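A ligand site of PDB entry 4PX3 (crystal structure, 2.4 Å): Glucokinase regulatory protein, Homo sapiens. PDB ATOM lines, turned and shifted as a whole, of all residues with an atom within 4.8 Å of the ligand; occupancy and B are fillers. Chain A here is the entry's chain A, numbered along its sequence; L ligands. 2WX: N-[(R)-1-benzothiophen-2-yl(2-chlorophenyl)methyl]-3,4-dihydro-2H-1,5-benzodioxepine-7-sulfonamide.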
ATOM      1  N   HIS A  21     -14.673 -10.773 -16.968  1.00  0.00           N
ATOM      2  CA  HIS A  21     -15.194  -9.395 -16.878  1.00  0.00           C
ATOM      3  C   HIS A  21     -15.691  -8.932 -15.504  1.00  0.00           C
ATOM      4  O   HIS A  21     -16.013  -7.757 -15.338  1.00  0.00           O
ATOM      5  CB  HIS A  21     -16.358  -9.245 -17.868  1.00  0.00           C
ATOM      6  CG  HIS A  21     -17.573 -10.028 -17.474  1.00  0.00           C
ATOM      7  ND1 HIS A  21     -17.769 -11.339 -17.858  1.00  0.00           N
ATOM      8  CD2 HIS A  21     -18.599  -9.719 -16.650  1.00  0.00           C
ATOM      9  CE1 HIS A  21     -18.885 -11.788 -17.320  1.00  0.00           C
ATOM     10  NE2 HIS A  21     -19.410 -10.825 -16.576  1.00  0.00           N
ATOM     11  N   VAL A  22     -15.767  -9.819 -14.507  1.00  0.00           N
ATOM     12  CA  VAL A  22     -16.273  -9.383 -13.188  1.00  0.00           C
ATOM     13  C   VAL A  22     -15.191  -8.619 -12.460  1.00  0.00           C
ATOM     14  O   VAL A  22     -14.075  -9.064 -12.430  1.00  0.00           O
ATOM     15  CB  VAL A  22     -16.767 -10.579 -12.331  1.00  0.00           C
ATOM     16  CG1 VAL A  22     -17.311 -10.132 -10.977  1.00  0.00           C
ATOM     17  CG2 VAL A  22     -17.847 -11.359 -13.084  1.00  0.00           C
ATOM     18  N   ILE A  23     -15.512  -7.483 -11.868  1.00  0.00           N
ATOM     19  CA  ILE A  23     -14.568  -6.683 -11.080  1.00  0.00           C
ATOM     20  C   ILE A  23     -14.506  -7.215  -9.648  1.00  0.00           C
ATOM     21  O   ILE A  23     -15.534  -7.554  -9.084  1.00  0.00           O
ATOM     22  CB  ILE A  23     -15.005  -5.191 -10.949  1.00  0.00           C
ATOM     23  CG1 ILE A  23     -15.261  -4.553 -12.306  1.00  0.00           C
ATOM     24  CG2 ILE A  23     -13.944  -4.374 -10.217  1.00  0.00           C
ATOM     25  CD1 ILE A  23     -14.078  -4.632 -13.261  1.00  0.00           C
ATOM     26  N   TYR A  36     -14.472   0.753  -8.698  1.00  0.00           N
ATOM     27  CA  TYR A  36     -15.576  -0.172  -8.937  1.00  0.00           C
ATOM     28  C   TYR A  36     -16.865   0.656  -9.150  1.00  0.00           C
ATOM     29  O   TYR A  36     -17.587   0.414 -10.117  1.00  0.00           O
ATOM     30  CB  TYR A  36     -15.742  -1.111  -7.752  1.00  0.00           C
ATOM     31  CG  TYR A  36     -16.874  -2.123  -7.796  1.00  0.00           C
ATOM     32  CD1 TYR A  36     -18.192  -1.751  -7.529  1.00  0.00           C
ATOM     33  CD2 TYR A  36     -16.614  -3.446  -8.019  1.00  0.00           C
ATOM     34  CE1 TYR A  36     -19.229  -2.696  -7.519  1.00  0.00           C
ATOM     35  CE2 TYR A  36     -17.621  -4.391  -8.003  1.00  0.00           C
ATOM     36  CZ  TYR A  36     -18.934  -4.004  -7.761  1.00  0.00           C
ATOM     37  OH  TYR A  36     -19.941  -4.949  -7.745  1.00  0.00           O
ATOM     38  N   ALA A  39     -17.483   2.035 -12.489  1.00  0.00           N
ATOM     39  CA  ALA A  39     -17.867   1.055 -13.469  1.00  0.00           C
ATOM     40  C   ALA A  39     -19.340   0.571 -13.388  1.00  0.00           C
ATOM     41  O   ALA A  39     -19.816  -0.039 -14.354  1.00  0.00           O
ATOM     42  CB  ALA A  39     -16.951  -0.137 -13.357  1.00  0.00           C
ATOM     43  N   VAL A  40     -20.035   0.821 -12.275  1.00  0.00           N
ATOM     44  CA  VAL A  40     -21.454   0.387 -12.151  1.00  0.00           C
ATOM     45  C   VAL A  40     -22.230   1.187 -13.131  1.00  0.00           C
ATOM     46  O   VAL A  40     -22.230   2.420 -13.056  1.00  0.00           O
ATOM     47  CB  VAL A  40     -22.004   0.596 -10.731  1.00  0.00           C
ATOM     48  CG1 VAL A  40     -23.473   0.139 -10.603  1.00  0.00           C
ATOM     49  CG2 VAL A  40     -21.147  -0.167  -9.714  1.00  0.00           C
ATOM     50  N   PRO A  41     -22.879   0.529 -14.104  1.00  0.00           N
ATOM     51  CA  PRO A  41     -23.716   1.317 -15.049  1.00  0.00           C
ATOM     52  C   PRO A  41     -24.758   2.167 -14.313  1.00  0.00           C
ATOM     53  O   PRO A  41     -25.288   1.745 -13.257  1.00  0.00           O
ATOM     54  CB  PRO A  41     -24.371   0.238 -15.925  1.00  0.00           C
ATOM     55  CG  PRO A  41     -23.421  -0.962 -15.834  1.00  0.00           C
ATOM     56  CD  PRO A  41     -22.802  -0.895 -14.472  1.00  0.00           C
ATOM     57  N   THR A  43     -27.766   2.643 -14.928  1.00  0.00           N
ATOM     58  CA  THR A  43     -29.046   1.947 -14.837  1.00  0.00           C
ATOM     59  C   THR A  43     -29.041   0.886 -13.751  1.00  0.00           C
ATOM     60  O   THR A  43     -30.060   0.453 -13.339  1.00  0.00           O
ATOM     61  CB  THR A  43     -29.428   1.310 -16.185  1.00  0.00           C
ATOM     62  OG1 THR A  43     -28.466   0.311 -16.573  1.00  0.00           O
ATOM     63  CG2 THR A  43     -29.451   2.373 -17.238  1.00  0.00           C
ATOM     64  N   GLU A  44     -27.860   0.449 -13.316  1.00  0.00           N
ATOM     65  CA  GLU A  44     -27.749  -0.462 -12.187  1.00  0.00           C
ATOM     66  C   GLU A  44     -27.367   0.236 -10.868  1.00  0.00           C
ATOM     67  O   GLU A  44     -27.373  -0.381  -9.845  1.00  0.00           O
ATOM     68  CB  GLU A  44     -26.745  -1.566 -12.503  1.00  0.00           C
ATOM     69  CG  GLU A  44     -27.140  -2.445 -13.689  1.00  0.00           C
ATOM     70  CD  GLU A  44     -28.290  -3.444 -13.443  1.00  0.00           C
ATOM     71  OE1 GLU A  44     -28.378  -4.108 -12.386  1.00  0.00           O
ATOM     72  OE2 GLU A  44     -29.163  -3.573 -14.312  1.00  0.00           O
ATOM     73  N   GLY A 193     -30.563  -0.431 -20.562  1.00  0.00           N
ATOM     74  CA  GLY A 193     -29.256  -0.671 -20.011  1.00  0.00           C
ATOM     75  C   GLY A 193     -28.210  -0.894 -21.061  1.00  0.00           C
ATOM     76  O   GLY A 193     -27.066  -1.100 -20.714  1.00  0.00           O
ATOM     77  N   LEU A 194     -28.575  -0.801 -22.338  1.00  0.00           N
ATOM     78  CA  LEU A 194     -27.632  -1.095 -23.473  1.00  0.00           C
ATOM     79  C   LEU A 194     -27.060  -2.517 -23.177  1.00  0.00           C
ATOM     80  O   LEU A 194     -25.883  -2.735 -22.955  1.00  0.00           O
ATOM     81  CB  LEU A 194     -26.541  -0.054 -23.622  1.00  0.00           C
ATOM     82  CG  LEU A 194     -26.790   1.426 -24.068  1.00  0.00           C
ATOM     83  CD1 LEU A 194     -25.488   2.072 -24.536  1.00  0.00           C
ATOM     84  CD2 LEU A 194     -27.766   1.564 -25.181  1.00  0.00           C
ATOM     85  N   SER A 195     -27.990  -3.446 -23.135  1.00  0.00           N
ATOM     86  CA  SER A 195     -27.841  -4.627 -22.399  1.00  0.00           C
ATOM     87  C   SER A 195     -28.371  -5.866 -23.127  1.00  0.00           C
ATOM     88  O   SER A 195     -27.758  -6.926 -22.990  1.00  0.00           O
ATOM     89  CB  SER A 195     -28.602  -4.466 -21.068  1.00  0.00           C
ATOM     90  OG  SER A 195     -28.845  -5.731 -20.515  1.00  0.00           O
ATOM     91  N   ASN A 221     -27.469   4.465 -20.849  1.00  0.00           N
ATOM     92  CA  ASN A 221     -26.127   4.408 -20.292  1.00  0.00           C
ATOM     93  C   ASN A 221     -25.135   5.009 -21.279  1.00  0.00           C
ATOM     94  O   ASN A 221     -25.330   4.957 -22.471  1.00  0.00           O
ATOM     95  CB  ASN A 221     -25.712   2.989 -20.044  1.00  0.00           C
ATOM     96  CG  ASN A 221     -26.173   2.471 -18.735  1.00  0.00           C
ATOM     97  OD1 ASN A 221     -26.127   3.177 -17.753  1.00  0.00           O
ATOM     98  ND2 ASN A 221     -26.598   1.219 -18.689  1.00  0.00           N
ATOM     99  N   MET A 225     -20.362   2.041 -20.596  1.00  0.00           N
ATOM    100  CA  MET A 225     -20.911   1.127 -19.568  1.00  0.00           C
ATOM    101  C   MET A 225     -21.842   0.083 -20.151  1.00  0.00           C
ATOM    102  O   MET A 225     -22.457  -0.677 -19.420  1.00  0.00           O
ATOM    103  CB  MET A 225     -21.710   1.914 -18.537  1.00  0.00           C
ATOM    104  CG  MET A 225     -20.888   2.662 -17.508  1.00  0.00           C
ATOM    105  SD  MET A 225     -21.901   4.055 -16.873  1.00  0.00           S
ATOM    106  CE  MET A 225     -20.882   4.630 -15.530  1.00  0.00           C
ATOM    107  N   ALA A 226     -22.021   0.080 -21.464  1.00  0.00           N
ATOM    108  CA  ALA A 226     -22.743  -0.967 -22.123  1.00  0.00           C
ATOM    109  C   ALA A 226     -22.206  -2.307 -21.684  1.00  0.00           C
ATOM    110  O   ALA A 226     -21.028  -2.450 -21.399  1.00  0.00           O
ATOM    111  CB  ALA A 226     -22.519  -0.817 -23.602  1.00  0.00           C
ATOM    112  N   ARG A 227     -23.066  -3.321 -21.644  1.00  0.00           N
ATOM    113  CA  ARG A 227     -22.602  -4.695 -21.398  1.00  0.00           C
ATOM    114  C   ARG A 227     -21.453  -5.165 -22.283  1.00  0.00           C
ATOM    115  O   ARG A 227     -21.490  -4.972 -23.513  1.00  0.00           O
ATOM    116  CB  ARG A 227     -23.739  -5.674 -21.518  1.00  0.00           C
ATOM    117  CG  ARG A 227     -24.585  -5.572 -20.293  1.00  0.00           C
ATOM    118  CD  ARG A 227     -25.689  -6.556 -20.235  1.00  0.00           C
ATOM    119  NE  ARG A 227     -25.213  -7.927 -20.135  1.00  0.00           N
ATOM    120  CZ  ARG A 227     -26.046  -8.967 -20.113  1.00  0.00           C
ATOM    121  NH1 ARG A 227     -27.358  -8.765 -20.187  1.00  0.00           N
ATOM    122  NH2 ARG A 227     -25.567 -10.208 -20.016  1.00  0.00           N
ATOM    123  N   ASN A 228     -20.446  -5.780 -21.645  1.00  0.00           N
ATOM    124  CA  ASN A 228     -19.268  -6.313 -22.308  1.00  0.00           C
ATOM    125  C   ASN A 228     -18.991  -7.780 -21.971  1.00  0.00           C
ATOM    126  O   ASN A 228     -17.889  -8.193 -22.116  1.00  0.00           O
ATOM    127  CB  ASN A 228     -18.038  -5.449 -21.984  1.00  0.00           C
ATOM    128  CG  ASN A 228     -16.898  -5.618 -22.992  1.00  0.00           C
ATOM    129  OD1 ASN A 228     -17.106  -5.701 -24.201  1.00  0.00           O
ATOM    130  ND2 ASN A 228     -15.680  -5.652 -22.489  1.00  0.00           N
ATOM    131  N   ASP A 229     -19.993  -8.538 -21.549  1.00  0.00           N
ATOM    132  CA  ASP A 229     -19.848  -9.934 -21.256  1.00  0.00           C
ATOM    133  C   ASP A 229     -20.313 -10.651 -22.505  1.00  0.00           C
ATOM    134  O   ASP A 229     -21.071 -10.075 -23.269  1.00  0.00           O
ATOM    135  CB  ASP A 229     -20.708 -10.362 -20.019  1.00  0.00           C
ATOM    136  CG  ASP A 229     -22.241 -10.247 -20.250  1.00  0.00           C
ATOM    137  OD1 ASP A 229     -22.620  -9.278 -20.927  1.00  0.00           O
ATOM    138  OD2 ASP A 229     -23.073 -11.068 -19.711  1.00  0.00           O
ATOM    139  N   LYS A 526     -28.586 -10.856 -17.356  1.00  0.00           N
ATOM    140  CA  LYS A 526     -28.503  -9.566 -16.663  1.00  0.00           C
ATOM    141  C   LYS A 526     -28.821  -9.664 -15.171  1.00  0.00           C
ATOM    142  O   LYS A 526     -28.112  -9.120 -14.335  1.00  0.00           O
ATOM    143  CB  LYS A 526     -29.404  -8.518 -17.330  1.00  0.00           C
ATOM    144  CG  LYS A 526     -29.499  -7.196 -16.576  1.00  0.00           C
ATOM    145  CD  LYS A 526     -30.244  -6.112 -17.355  1.00  0.00           C
ATOM    146  CE  LYS A 526     -31.740  -6.427 -17.432  1.00  0.00           C
ATOM    147  NZ  LYS A 526     -32.341  -5.527 -18.425  1.00  0.00           N
ATOM    148  N   TRP A 529     -26.129 -11.236 -13.249  1.00  0.00           N
ATOM    149  CA  TRP A 529     -25.095 -10.295 -12.828  1.00  0.00           C
ATOM    150  C   TRP A 529     -25.522  -9.379 -11.726  1.00  0.00           C
ATOM    151  O   TRP A 529     -24.680  -9.001 -10.889  1.00  0.00           O
ATOM    152  CB  TRP A 529     -24.560  -9.465 -13.994  1.00  0.00           C
ATOM    153  CG  TRP A 529     -24.033 -10.310 -15.079  1.00  0.00           C
ATOM    154  CD1 TRP A 529     -24.438 -10.321 -16.353  1.00  0.00           C
ATOM    155  CD2 TRP A 529     -23.025 -11.300 -14.970  1.00  0.00           C
ATOM    156  NE1 TRP A 529     -23.734 -11.245 -17.071  1.00  0.00           N
ATOM    157  CE2 TRP A 529     -22.857 -11.871 -16.241  1.00  0.00           C
ATOM    158  CE3 TRP A 529     -22.190 -11.710 -13.935  1.00  0.00           C
ATOM    159  CZ2 TRP A 529     -21.895 -12.862 -16.512  1.00  0.00           C
ATOM    160  CZ3 TRP A 529     -21.237 -12.747 -14.181  1.00  0.00           C
ATOM    161  CH2 TRP A 529     -21.109 -13.294 -15.474  1.00  0.00           C
ATOM    162  N   LEU A 532     -25.147 -11.267  -8.552  1.00  0.00           N
ATOM    163  CA  LEU A 532     -23.747 -11.306  -8.145  1.00  0.00           C
ATOM    164  C   LEU A 532     -23.314  -9.972  -7.549  1.00  0.00           C
ATOM    165  O   LEU A 532     -22.681  -9.946  -6.523  1.00  0.00           O
ATOM    166  CB  LEU A 532     -22.865 -11.707  -9.286  1.00  0.00           C
ATOM    167  CG  LEU A 532     -21.357 -11.762  -9.024  1.00  0.00           C
ATOM    168  CD1 LEU A 532     -21.091 -12.746  -7.876  1.00  0.00           C
ATOM    169  CD2 LEU A 532     -20.612 -12.209 -10.264  1.00  0.00           C
ATOM    170  N   ALA A 533     -23.645  -8.862  -8.185  1.00  0.00           N
ATOM    171  CA  ALA A 533     -23.323  -7.543  -7.630  1.00  0.00           C
ATOM    172  C   ALA A 533     -23.980  -7.302  -6.284  1.00  0.00           C
ATOM    173  O   ALA A 533     -23.410  -6.668  -5.394  1.00  0.00           O
ATOM    174  CB  ALA A 533     -23.758  -6.443  -8.588  1.00  0.00           C
ATOM    175  N   GLN A 536     -21.709  -9.134  -3.764  1.00  0.00           N
ATOM    176  CA  GLN A 536     -20.533  -8.314  -3.447  1.00  0.00           C
ATOM    177  C   GLN A 536     -20.882  -7.113  -2.543  1.00  0.00           C
ATOM    178  O   GLN A 536     -20.120  -6.780  -1.650  1.00  0.00           O
ATOM    179  CB  GLN A 536     -19.844  -7.782  -4.692  1.00  0.00           C
ATOM    180  CG  GLN A 536     -19.575  -8.800  -5.756  1.00  0.00           C
ATOM    181  CD  GLN A 536     -18.755  -8.200  -6.851  1.00  0.00           C
ATOM    182  OE1 GLN A 536     -19.292  -7.538  -7.727  1.00  0.00           O
ATOM    183  NE2 GLN A 536     -17.442  -8.322  -6.759  1.00  0.00           N
HETATM  184  C18 2WX L   1     -21.761  -4.484 -14.903  1.00  0.00           C
HETATM  185  C20 2WX L   1     -21.512  -4.168 -13.641  1.00  0.00           C
HETATM  186  C21 2WX L   1     -20.303  -3.631 -13.157  1.00  0.00           C
HETATM  187  C22 2WX L   1     -20.192  -3.295 -11.801  1.00  0.00           C
HETATM  188  C23 2WX L   1     -21.332  -3.520 -10.975  1.00  0.00           C
HETATM  189  C24 2WX L   1     -22.548  -4.041 -11.443  1.00  0.00           C
HETATM  190  C19 2WX L   1     -22.628  -4.364 -12.781  1.00  0.00           C
HETATM  191  S2  2WX L   1     -23.871  -4.993 -13.694  1.00  0.00           S
HETATM  192  C3  2WX L   1     -22.955  -4.980 -15.171  1.00  0.00           C
HETATM  193  C1  2WX L   1     -23.361  -5.474 -16.576  1.00  0.00           C
HETATM  194  C2  2WX L   1     -24.410  -4.549 -17.108  1.00  0.00           C
HETATM  195  C4  2WX L   1     -24.113  -3.390 -17.898  1.00  0.00           C
HETATM  196  C5  2WX L   1     -25.131  -2.536 -18.384  1.00  0.00           C
HETATM  197  C6  2WX L   1     -26.447  -2.892 -18.058  1.00  0.00           C
HETATM  198  C7  2WX L   1     -26.731  -4.039 -17.298  1.00  0.00           C
HETATM  199  C8  2WX L   1     -25.722  -4.901 -16.819  1.00  0.00           C
HETATM  200 CL1  2WX L   1     -26.023  -6.373 -15.876  1.00  0.00          CL
HETATM  201  N1  2WX L   1     -22.239  -5.475 -17.548  1.00  0.00           N
HETATM  202  S1  2WX L   1     -21.255  -6.798 -17.649  1.00  0.00           S
HETATM  203  O1  2WX L   1     -20.326  -6.414 -18.779  1.00  0.00           O
HETATM  204  O2  2WX L   1     -22.111  -7.988 -17.927  1.00  0.00           O
HETATM  205  C9  2WX L   1     -20.403  -6.956 -16.058  1.00  0.00           C
HETATM  206  C10 2WX L   1     -21.005  -7.741 -15.058  1.00  0.00           C
HETATM  207  C13 2WX L   1     -20.425  -7.841 -13.803  1.00  0.00           C
HETATM  208  O4  2WX L   1     -21.124  -8.643 -12.945  1.00  0.00           O
HETATM  209  C16 2WX L   1     -21.533  -7.930 -11.766  1.00  0.00           C
HETATM  210  C17 2WX L   1     -20.454  -7.701 -10.695  1.00  0.00           C
HETATM  211  C15 2WX L   1     -19.328  -6.751 -11.164  1.00  0.00           C
HETATM  212  O3  2WX L   1     -18.548  -7.196 -12.307  1.00  0.00           O
HETATM  213  C14 2WX L   1     -19.227  -7.158 -13.522  1.00  0.00           C
HETATM  214  C11 2WX L   1     -18.594  -6.360 -14.504  1.00  0.00           C
HETATM  215  C12 2WX L   1     -19.196  -6.264 -15.769  1.00  0.00           C
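The backbone NH (N) of Asn 228 lies within hydrogen-bond range of an oxygen (O1) of the ligand (2.9 Å). The backbone NH of Ile 23 lies within hydrogen-bond range of an oxygen (O3) of the ligand (3.1 Å).
The side-chain carboxylate of Asp 229 lies close to an oxygen (O2) of the ligand (3.3 Å). His 21 touches the ligand. Val 22 touches the ligand. OH of Tyr 36 touches C23 of the ligand, at 3.8 Å. Ala 39 touches the ligand (O to C21, 3.8 Å). CG2 of Val 40 touches C23 of the ligand (3.6 Å). Pro 41 touches the ligand. Glu 44 touches the ligand (OE2 to C7, 3.9 Å). Gly 193 touches the ligand (O to C6, 3.3 Å). Met 225 touches the ligand. Arg 227 touches the ligand (CG to C4, 3.3 Å). Lys 526 touches the ligand (CG to CL1, 3.6 Å). Trp 529 touches the ligand. CB of Ala 533 touches C24 of the ligand, 3.9 Å away. OE1 of Gln 536 touches C17 of the ligand, at 3.2 Å. Hydrophobic or aromatic side chains that line the ligand: His 21, Val 22, Val 40, Pro 41, Trp 529 and Ala 533. Within 4 Å of the ligand: His 21, Val 22, Ile 23, Tyr 36, Ala 39, Val 40, Pro 41, Glu 44, Gly 193, Met 225, Arg 227, Asn 228, Asp 229, Lys 526, Trp 529, Ala 533 and Gln 536.
The side-chain amide nitrogen of Gln 536 lies within hydrogen-bond range of the backbone carbonyl oxygen of Ile 23 (3.1 Å). The side-chain amide oxygen (OE1) of Gln 536 is in hydrogen-bond range of the side-chain hydroxyl (OH) of Tyr 36 (2.7 Å). The side-chain carboxylate (OD2) of Asp 229 is in salt-bridge range of the guanidinium group (NH2) of Arg 227 (2.7 Å). OD2 of Asp 229 lies within hydrogen-bond range of NE1 of Trp 529, 2.7 Å away. O of Gly 193 sits at hydrogen-bond distance from ND2 of Asn 221 (3.1 Å). The guanidinium group (NH1) of Arg 227 sits at hydrogen-bond distance from the backbone carbonyl oxygen (O) of Ser 195. O of Leu 194 sits at hydrogen-bond distance from N of Arg 227, at 3.2 Å.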
